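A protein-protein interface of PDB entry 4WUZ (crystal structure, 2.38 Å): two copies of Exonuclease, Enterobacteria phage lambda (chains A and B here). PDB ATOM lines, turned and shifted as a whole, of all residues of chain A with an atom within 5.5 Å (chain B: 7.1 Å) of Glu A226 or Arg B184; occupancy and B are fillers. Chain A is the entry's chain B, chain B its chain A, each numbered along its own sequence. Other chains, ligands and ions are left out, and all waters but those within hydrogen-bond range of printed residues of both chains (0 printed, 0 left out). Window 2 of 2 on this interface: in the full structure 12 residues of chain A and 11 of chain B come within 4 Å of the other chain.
Printed residues of chain B within 4 Å of Cys A69: Met B182 (3.8 Å) and Lys B183 (3.0 Å).
Of the printed residues of chain B, Gly A221 touches Arg B184.
Printed residues of chain B within 4 Å of Phe A222: Arg B184 (3.3 Å).
Glu A226 touches one residue of chain B.
Gln A227 touches none of the printed residues of chain B.
Of the printed residues of chain A, Met B182 touches Cys A69.
Of the printed residues of chain A, Lys B183 touches Cys A69.
Of the printed residues of chain A, Arg B184 touches Gly A221, Phe A222 and Glu A226.
The nearest residue of chain A that does not touch Arg B184 is Val A223 (5.0 Å).
No position is printed for both chains.
Of the 5 pairs that touch across the chains among the printed residues, none has its exchanged pair printed and touching as well.
N of Lys B183 is in hydrogen-bond range of O of Cys A69 (3.0 Å).
The guanidinium group of Arg B184 sits at hydrogen-bond distance from the backbone carbonyl oxygen of Gly A221, 2.8 Å away.
The side-chain carboxylate (OE1) of Glu A226 lies within salt-bridge range of the guanidinium group (NH1) of Arg B184, 2.7 Å away.
CB of Cys A69 touches SD of Met B182, at 3.8 Å.
CD2 of Phe A222 touches NH2 of Arg B184 (3.3 Å).
OE2 of Glu A226 lies within hydrogen-bond range of N of Val A223 (2.6 Å).
Of the 10 printed residues of chain B, 3 touch a printed residue of chain A.
Hydrophobic or aromatic side chains of chain B within 4 Å of the printed part of chain A: Met B182.
Among the printed residues, 5 pairs touch across the chains.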
ATOM      1  N   VAL A  68     -22.806  -4.314 -21.061  1.00  0.00           N
ATOM      2  CA  VAL A  68     -21.624  -3.765 -21.755  1.00  0.00           C
ATOM      3  C   VAL A  68     -20.427  -3.432 -20.848  1.00  0.00           C
ATOM      4  O   VAL A  68     -19.269  -3.685 -21.210  1.00  0.00           O
ATOM      5  CB  VAL A  68     -21.941  -2.574 -22.588  1.00  0.00           C
ATOM      6  CG1 VAL A  68     -20.641  -2.066 -23.289  1.00  0.00           C
ATOM      7  CG2 VAL A  68     -23.002  -2.929 -23.644  1.00  0.00           C
ATOM      8  N   CYS A  69     -20.665  -2.854 -19.679  1.00  0.00           N
ATOM      9  CA  CYS A  69     -19.554  -2.307 -18.894  1.00  0.00           C
ATOM     10  C   CYS A  69     -18.972  -3.305 -17.890  1.00  0.00           C
ATOM     11  O   CYS A  69     -17.924  -3.040 -17.358  1.00  0.00           O
ATOM     12  CB  CYS A  69     -19.992  -1.067 -18.155  1.00  0.00           C
ATOM     13  SG  CYS A  69     -20.669   0.165 -19.233  1.00  0.00           S
ATOM     14  N   GLY A 221     -17.876   6.873 -20.588  1.00  0.00           N
ATOM     15  CA  GLY A 221     -16.555   6.500 -21.156  1.00  0.00           C
ATOM     16  C   GLY A 221     -16.365   5.048 -21.572  1.00  0.00           C
ATOM     17  O   GLY A 221     -15.240   4.551 -21.663  1.00  0.00           O
ATOM     18  N   PHE A 222     -17.488   4.383 -21.873  1.00  0.00           N
ATOM     19  CA  PHE A 222     -17.497   3.036 -22.450  1.00  0.00           C
ATOM     20  C   PHE A 222     -17.961   3.060 -23.883  1.00  0.00           C
ATOM     21  O   PHE A 222     -18.601   4.046 -24.344  1.00  0.00           O
ATOM     22  CB  PHE A 222     -18.453   2.162 -21.634  1.00  0.00           C
ATOM     23  CG  PHE A 222     -17.837   1.601 -20.394  1.00  0.00           C
ATOM     24  CD1 PHE A 222     -17.898   2.298 -19.216  1.00  0.00           C
ATOM     25  CD2 PHE A 222     -17.195   0.369 -20.414  1.00  0.00           C
ATOM     26  CE1 PHE A 222     -17.348   1.805 -18.088  1.00  0.00           C
ATOM     27  CE2 PHE A 222     -16.615  -0.137 -19.265  1.00  0.00           C
ATOM     28  CZ  PHE A 222     -16.680   0.584 -18.099  1.00  0.00           C
ATOM     29  N   VAL A 223     -17.730   1.940 -24.566  1.00  0.00           N
ATOM     30  CA  VAL A 223     -18.217   1.792 -25.925  1.00  0.00           C
ATOM     31  C   VAL A 223     -18.874   0.394 -26.127  1.00  0.00           C
ATOM     32  O   VAL A 223     -18.395  -0.619 -25.570  1.00  0.00           O
ATOM     33  CB  VAL A 223     -17.062   2.140 -26.969  1.00  0.00           C
ATOM     34  CG1 VAL A 223     -15.872   1.276 -26.756  1.00  0.00           C
ATOM     35  CG2 VAL A 223     -17.533   2.005 -28.428  1.00  0.00           C
ATOM     36  N   PHE A 224     -19.953   0.327 -26.917  1.00  0.00           N
ATOM     37  CA  PHE A 224     -20.511  -0.994 -27.247  1.00  0.00           C
ATOM     38  C   PHE A 224     -19.489  -1.874 -27.907  1.00  0.00           C
ATOM     39  O   PHE A 224     -18.769  -1.418 -28.748  1.00  0.00           O
ATOM     40  CB  PHE A 224     -21.723  -0.940 -28.152  1.00  0.00           C
ATOM     41  CG  PHE A 224     -22.345  -2.324 -28.420  1.00  0.00           C
ATOM     42  CD1 PHE A 224     -23.273  -2.876 -27.524  1.00  0.00           C
ATOM     43  CD2 PHE A 224     -21.989  -3.064 -29.559  1.00  0.00           C
ATOM     44  CE1 PHE A 224     -23.843  -4.122 -27.769  1.00  0.00           C
ATOM     45  CE2 PHE A 224     -22.555  -4.320 -29.836  1.00  0.00           C
ATOM     46  CZ  PHE A 224     -23.482  -4.864 -28.944  1.00  0.00           C
ATOM     47  N   GLY A 225     -19.415  -3.147 -27.527  1.00  0.00           N
ATOM     48  CA  GLY A 225     -18.456  -4.055 -28.148  1.00  0.00           C
ATOM     49  C   GLY A 225     -17.384  -4.331 -27.152  1.00  0.00           C
ATOM     50  O   GLY A 225     -16.688  -5.358 -27.245  1.00  0.00           O
ATOM     51  N   GLU A 226     -17.261  -3.437 -26.160  1.00  0.00           N
ATOM     52  CA  GLU A 226     -16.293  -3.607 -25.078  1.00  0.00           C
ATOM     53  C   GLU A 226     -16.504  -4.908 -24.330  1.00  0.00           C
ATOM     54  O   GLU A 226     -15.603  -5.367 -23.633  1.00  0.00           O
ATOM     55  CB  GLU A 226     -16.366  -2.437 -24.079  1.00  0.00           C
ATOM     56  CG  GLU A 226     -15.205  -1.418 -24.219  1.00  0.00           C
ATOM     57  CD  GLU A 226     -15.178  -0.366 -23.120  1.00  0.00           C
ATOM     58  OE1 GLU A 226     -14.435  -0.532 -22.124  1.00  0.00           O
ATOM     59  OE2 GLU A 226     -15.863   0.668 -23.282  1.00  0.00           O
ATOM     60  N   GLN A 227     -17.691  -5.511 -24.447  1.00  0.00           N
ATOM     61  CA  GLN A 227     -17.979  -6.679 -23.646  1.00  0.00           C
ATOM     62  C   GLN A 227     -17.341  -7.892 -24.292  1.00  0.00           C
ATOM     63  O   GLN A 227     -17.139  -8.890 -23.630  1.00  0.00           O
ATOM     64  CB  GLN A 227     -19.485  -6.865 -23.444  1.00  0.00           C
ATOM     65  CG  GLN A 227     -20.278  -7.175 -24.702  1.00  0.00           C
ATOM     66  CD  GLN A 227     -20.720  -5.925 -25.423  1.00  0.00           C
ATOM     67  OE1 GLN A 227     -20.106  -4.841 -25.256  1.00  0.00           O
ATOM     68  NE2 GLN A 227     -21.770  -6.056 -26.265  1.00  0.00           N
ATOM     69  N   TRP A 228     -17.036  -7.766 -25.589  1.00  0.00           N
ATOM     70  CA  TRP A 228     -16.433  -8.820 -26.421  1.00  0.00           C
ATOM     71  C   TRP A 228     -14.918  -8.677 -26.606  1.00  0.00           C
ATOM     72  O   TRP A 228     -14.230  -9.635 -26.840  1.00  0.00           O
ATOM     73  CB  TRP A 228     -17.125  -8.901 -27.793  1.00  0.00           C
ATOM     74  CG  TRP A 228     -18.594  -9.224 -27.697  1.00  0.00           C
ATOM     75  CD1 TRP A 228     -19.193 -10.112 -26.831  1.00  0.00           C
ATOM     76  CD2 TRP A 228     -19.653  -8.660 -28.469  1.00  0.00           C
ATOM     77  NE1 TRP A 228     -20.543 -10.149 -27.034  1.00  0.00           N
ATOM     78  CE2 TRP A 228     -20.862  -9.257 -28.020  1.00  0.00           C
ATOM     79  CE3 TRP A 228     -19.709  -7.704 -29.505  1.00  0.00           C
ATOM     80  CZ2 TRP A 228     -22.105  -8.913 -28.539  1.00  0.00           C
ATOM     81  CZ3 TRP A 228     -20.979  -7.404 -30.068  1.00  0.00           C
ATOM     82  CH2 TRP A 228     -22.141  -8.023 -29.576  1.00  0.00           C
ATOM     83  N   ARG A 229     -14.400  -7.465 -26.471  1.00  0.00           N
ATOM     84  CA  ARG A 229     -12.956  -7.194 -26.488  1.00  0.00           C
ATOM     85  C   ARG A 229     -12.182  -8.234 -25.665  1.00  0.00           C
ATOM     86  O   ARG A 229     -12.592  -8.618 -24.546  1.00  0.00           O
ATOM     87  CB  ARG A 229     -12.672  -5.776 -25.970  1.00  0.00           C
ATOM     88  OXT ARG A 229     -11.128  -8.708 -26.129  1.00  0.00           O
ATOM     89  N   PHE B 142     -26.318  -0.396  -9.932  1.00  0.00           N
ATOM     90  CA  PHE B 142     -25.148   0.452  -9.929  1.00  0.00           C
ATOM     91  C   PHE B 142     -25.338   1.464 -11.044  1.00  0.00           C
ATOM     92  O   PHE B 142     -25.201   2.643 -10.828  1.00  0.00           O
ATOM     93  CB  PHE B 142     -23.851  -0.298 -10.179  1.00  0.00           C
ATOM     94  CG  PHE B 142     -22.660   0.605 -10.195  1.00  0.00           C
ATOM     95  CD1 PHE B 142     -22.050   0.960 -11.402  1.00  0.00           C
ATOM     96  CD2 PHE B 142     -22.208   1.191  -9.004  1.00  0.00           C
ATOM     97  CE1 PHE B 142     -20.977   1.820 -11.413  1.00  0.00           C
ATOM     98  CE2 PHE B 142     -21.111   2.058  -9.005  1.00  0.00           C
ATOM     99  CZ  PHE B 142     -20.492   2.374 -10.209  1.00  0.00           C
ATOM    100  N   ASP B 179     -19.433  -1.400  -7.234  1.00  0.00           N
ATOM    101  CA  ASP B 179     -19.660  -2.567  -8.058  1.00  0.00           C
ATOM    102  C   ASP B 179     -18.344  -3.166  -8.540  1.00  0.00           C
ATOM    103  O   ASP B 179     -17.738  -2.678  -9.493  1.00  0.00           O
ATOM    104  CB  ASP B 179     -20.504  -2.235  -9.276  1.00  0.00           C
ATOM    105  CG  ASP B 179     -20.990  -3.503 -10.008  1.00  0.00           C
ATOM    106  OD1 ASP B 179     -20.466  -4.622  -9.704  1.00  0.00           O
ATOM    107  OD2 ASP B 179     -21.908  -3.388 -10.867  1.00  0.00           O
ATOM    108  N   PRO B 180     -17.936  -4.267  -7.917  1.00  0.00           N
ATOM    109  CA  PRO B 180     -16.631  -4.848  -8.225  1.00  0.00           C
ATOM    110  C   PRO B 180     -16.588  -5.359  -9.652  1.00  0.00           C
ATOM    111  O   PRO B 180     -15.483  -5.496 -10.205  1.00  0.00           O
ATOM    112  CB  PRO B 180     -16.531  -6.038  -7.279  1.00  0.00           C
ATOM    113  CG  PRO B 180     -17.942  -6.336  -6.896  1.00  0.00           C
ATOM    114  CD  PRO B 180     -18.691  -5.045  -6.928  1.00  0.00           C
ATOM    115  N   ARG B 181     -17.771  -5.625 -10.242  1.00  0.00           N
ATOM    116  CA  ARG B 181     -17.885  -6.158 -11.617  1.00  0.00           C
ATOM    117  C   ARG B 181     -17.572  -5.165 -12.741  1.00  0.00           C
ATOM    118  O   ARG B 181     -17.174  -5.583 -13.834  1.00  0.00           O
ATOM    119  CB  ARG B 181     -19.253  -6.812 -11.838  1.00  0.00           C
ATOM    120  CG  ARG B 181     -19.432  -8.142 -11.068  1.00  0.00           C
ATOM    121  CD  ARG B 181     -20.872  -8.397 -10.698  1.00  0.00           C
ATOM    122  NE  ARG B 181     -21.380  -7.224  -9.993  1.00  0.00           N
ATOM    123  CZ  ARG B 181     -22.576  -7.125  -9.432  1.00  0.00           C
ATOM    124  NH1 ARG B 181     -23.459  -8.131  -9.497  1.00  0.00           N
ATOM    125  NH2 ARG B 181     -22.883  -5.995  -8.822  1.00  0.00           N
ATOM    126  N   MET B 182     -17.768  -3.873 -12.496  1.00  0.00           N
ATOM    127  CA  MET B 182     -17.546  -2.864 -13.540  1.00  0.00           C
ATOM    128  C   MET B 182     -16.088  -2.938 -13.900  1.00  0.00           C
ATOM    129  O   MET B 182     -15.249  -2.965 -12.990  1.00  0.00           O
ATOM    130  CB  MET B 182     -17.853  -1.457 -13.046  1.00  0.00           C
ATOM    131  CG  MET B 182     -19.298  -1.164 -12.882  1.00  0.00           C
ATOM    132  SD  MET B 182     -20.180  -0.843 -14.397  1.00  0.00           S
ATOM    133  CE  MET B 182     -19.442   0.746 -14.802  1.00  0.00           C
ATOM    134  N   LYS B 183     -15.774  -2.969 -15.200  1.00  0.00           N
ATOM    135  CA  LYS B 183     -14.371  -3.154 -15.636  1.00  0.00           C
ATOM    136  C   LYS B 183     -13.454  -2.015 -15.169  1.00  0.00           C
ATOM    137  O   LYS B 183     -12.254  -2.176 -15.030  1.00  0.00           O
ATOM    138  CB  LYS B 183     -14.269  -3.340 -17.154  1.00  0.00           C
ATOM    139  CG  LYS B 183     -14.761  -4.696 -17.612  1.00  0.00           C
ATOM    140  CD  LYS B 183     -13.748  -5.818 -17.246  1.00  0.00           C
ATOM    141  CE  LYS B 183     -14.462  -7.014 -16.605  1.00  0.00           C
ATOM    142  NZ  LYS B 183     -13.554  -8.192 -16.389  1.00  0.00           N
ATOM    143  N   ARG B 184     -14.044  -0.860 -14.957  1.00  0.00           N
ATOM    144  CA  ARG B 184     -13.314   0.268 -14.473  1.00  0.00           C
ATOM    145  C   ARG B 184     -14.377   1.278 -13.985  1.00  0.00           C
ATOM    146  O   ARG B 184     -15.518   1.257 -14.459  1.00  0.00           O
ATOM    147  CB  ARG B 184     -12.373   0.816 -15.598  1.00  0.00           C
ATOM    148  CG  ARG B 184     -13.079   1.694 -16.643  1.00  0.00           C
ATOM    149  CD  ARG B 184     -12.236   1.958 -17.891  1.00  0.00           C
ATOM    150  NE  ARG B 184     -13.138   2.398 -18.947  1.00  0.00           N
ATOM    151  CZ  ARG B 184     -13.537   1.600 -19.937  1.00  0.00           C
ATOM    152  NH1 ARG B 184     -13.059   0.347 -20.006  1.00  0.00           N
ATOM    153  NH2 ARG B 184     -14.404   2.043 -20.852  1.00  0.00           N
ATOM    154  N   GLU B 185     -13.996   2.157 -13.053  1.00  0.00           N
ATOM    155  CA  GLU B 185     -14.916   3.166 -12.470  1.00  0.00           C
ATOM    156  C   GLU B 185     -16.181   2.618 -11.784  1.00  0.00           C
ATOM    157  O   GLU B 185     -17.299   3.115 -12.018  1.00  0.00           O
ATOM    158  CB  GLU B 185     -15.344   4.177 -13.497  1.00  0.00           C
ATOM    159  CG  GLU B 185     -14.271   5.174 -13.886  1.00  0.00           C
ATOM    160  CD  GLU B 185     -14.667   5.884 -15.154  1.00  0.00           C
ATOM    161  OE1 GLU B 185     -13.791   6.005 -16.049  1.00  0.00           O
ATOM    162  OE2 GLU B 185     -15.875   6.260 -15.264  1.00  0.00           O
ATOM    163  N   GLY B 186     -15.966   1.636 -10.900  1.00  0.00           N
ATOM    164  CA  GLY B 186     -17.028   0.962 -10.155  1.00  0.00           C
ATOM    165  C   GLY B 186     -17.353   1.522  -8.770  1.00  0.00           C
ATOM    166  O   GLY B 186     -18.073   0.872  -7.986  1.00  0.00           O
ATOM    167  N   LEU B 187     -16.833   2.710  -8.460  1.00  0.00           N
ATOM    168  CA  LEU B 187     -17.299   3.490  -7.315  1.00  0.00           C
ATOM    169  C   LEU B 187     -17.824   4.775  -7.830  1.00  0.00           C
ATOM    170  O   LEU B 187     -17.123   5.468  -8.529  1.00  0.00           O
ATOM    171  CB  LEU B 187     -16.159   3.834  -6.373  1.00  0.00           C
ATOM    172  CG  LEU B 187     -16.617   4.581  -5.117  1.00  0.00           C
ATOM    173  CD1 LEU B 187     -17.410   3.651  -4.229  1.00  0.00           C
ATOM    174  CD2 LEU B 187     -15.418   5.098  -4.365  1.00  0.00           C
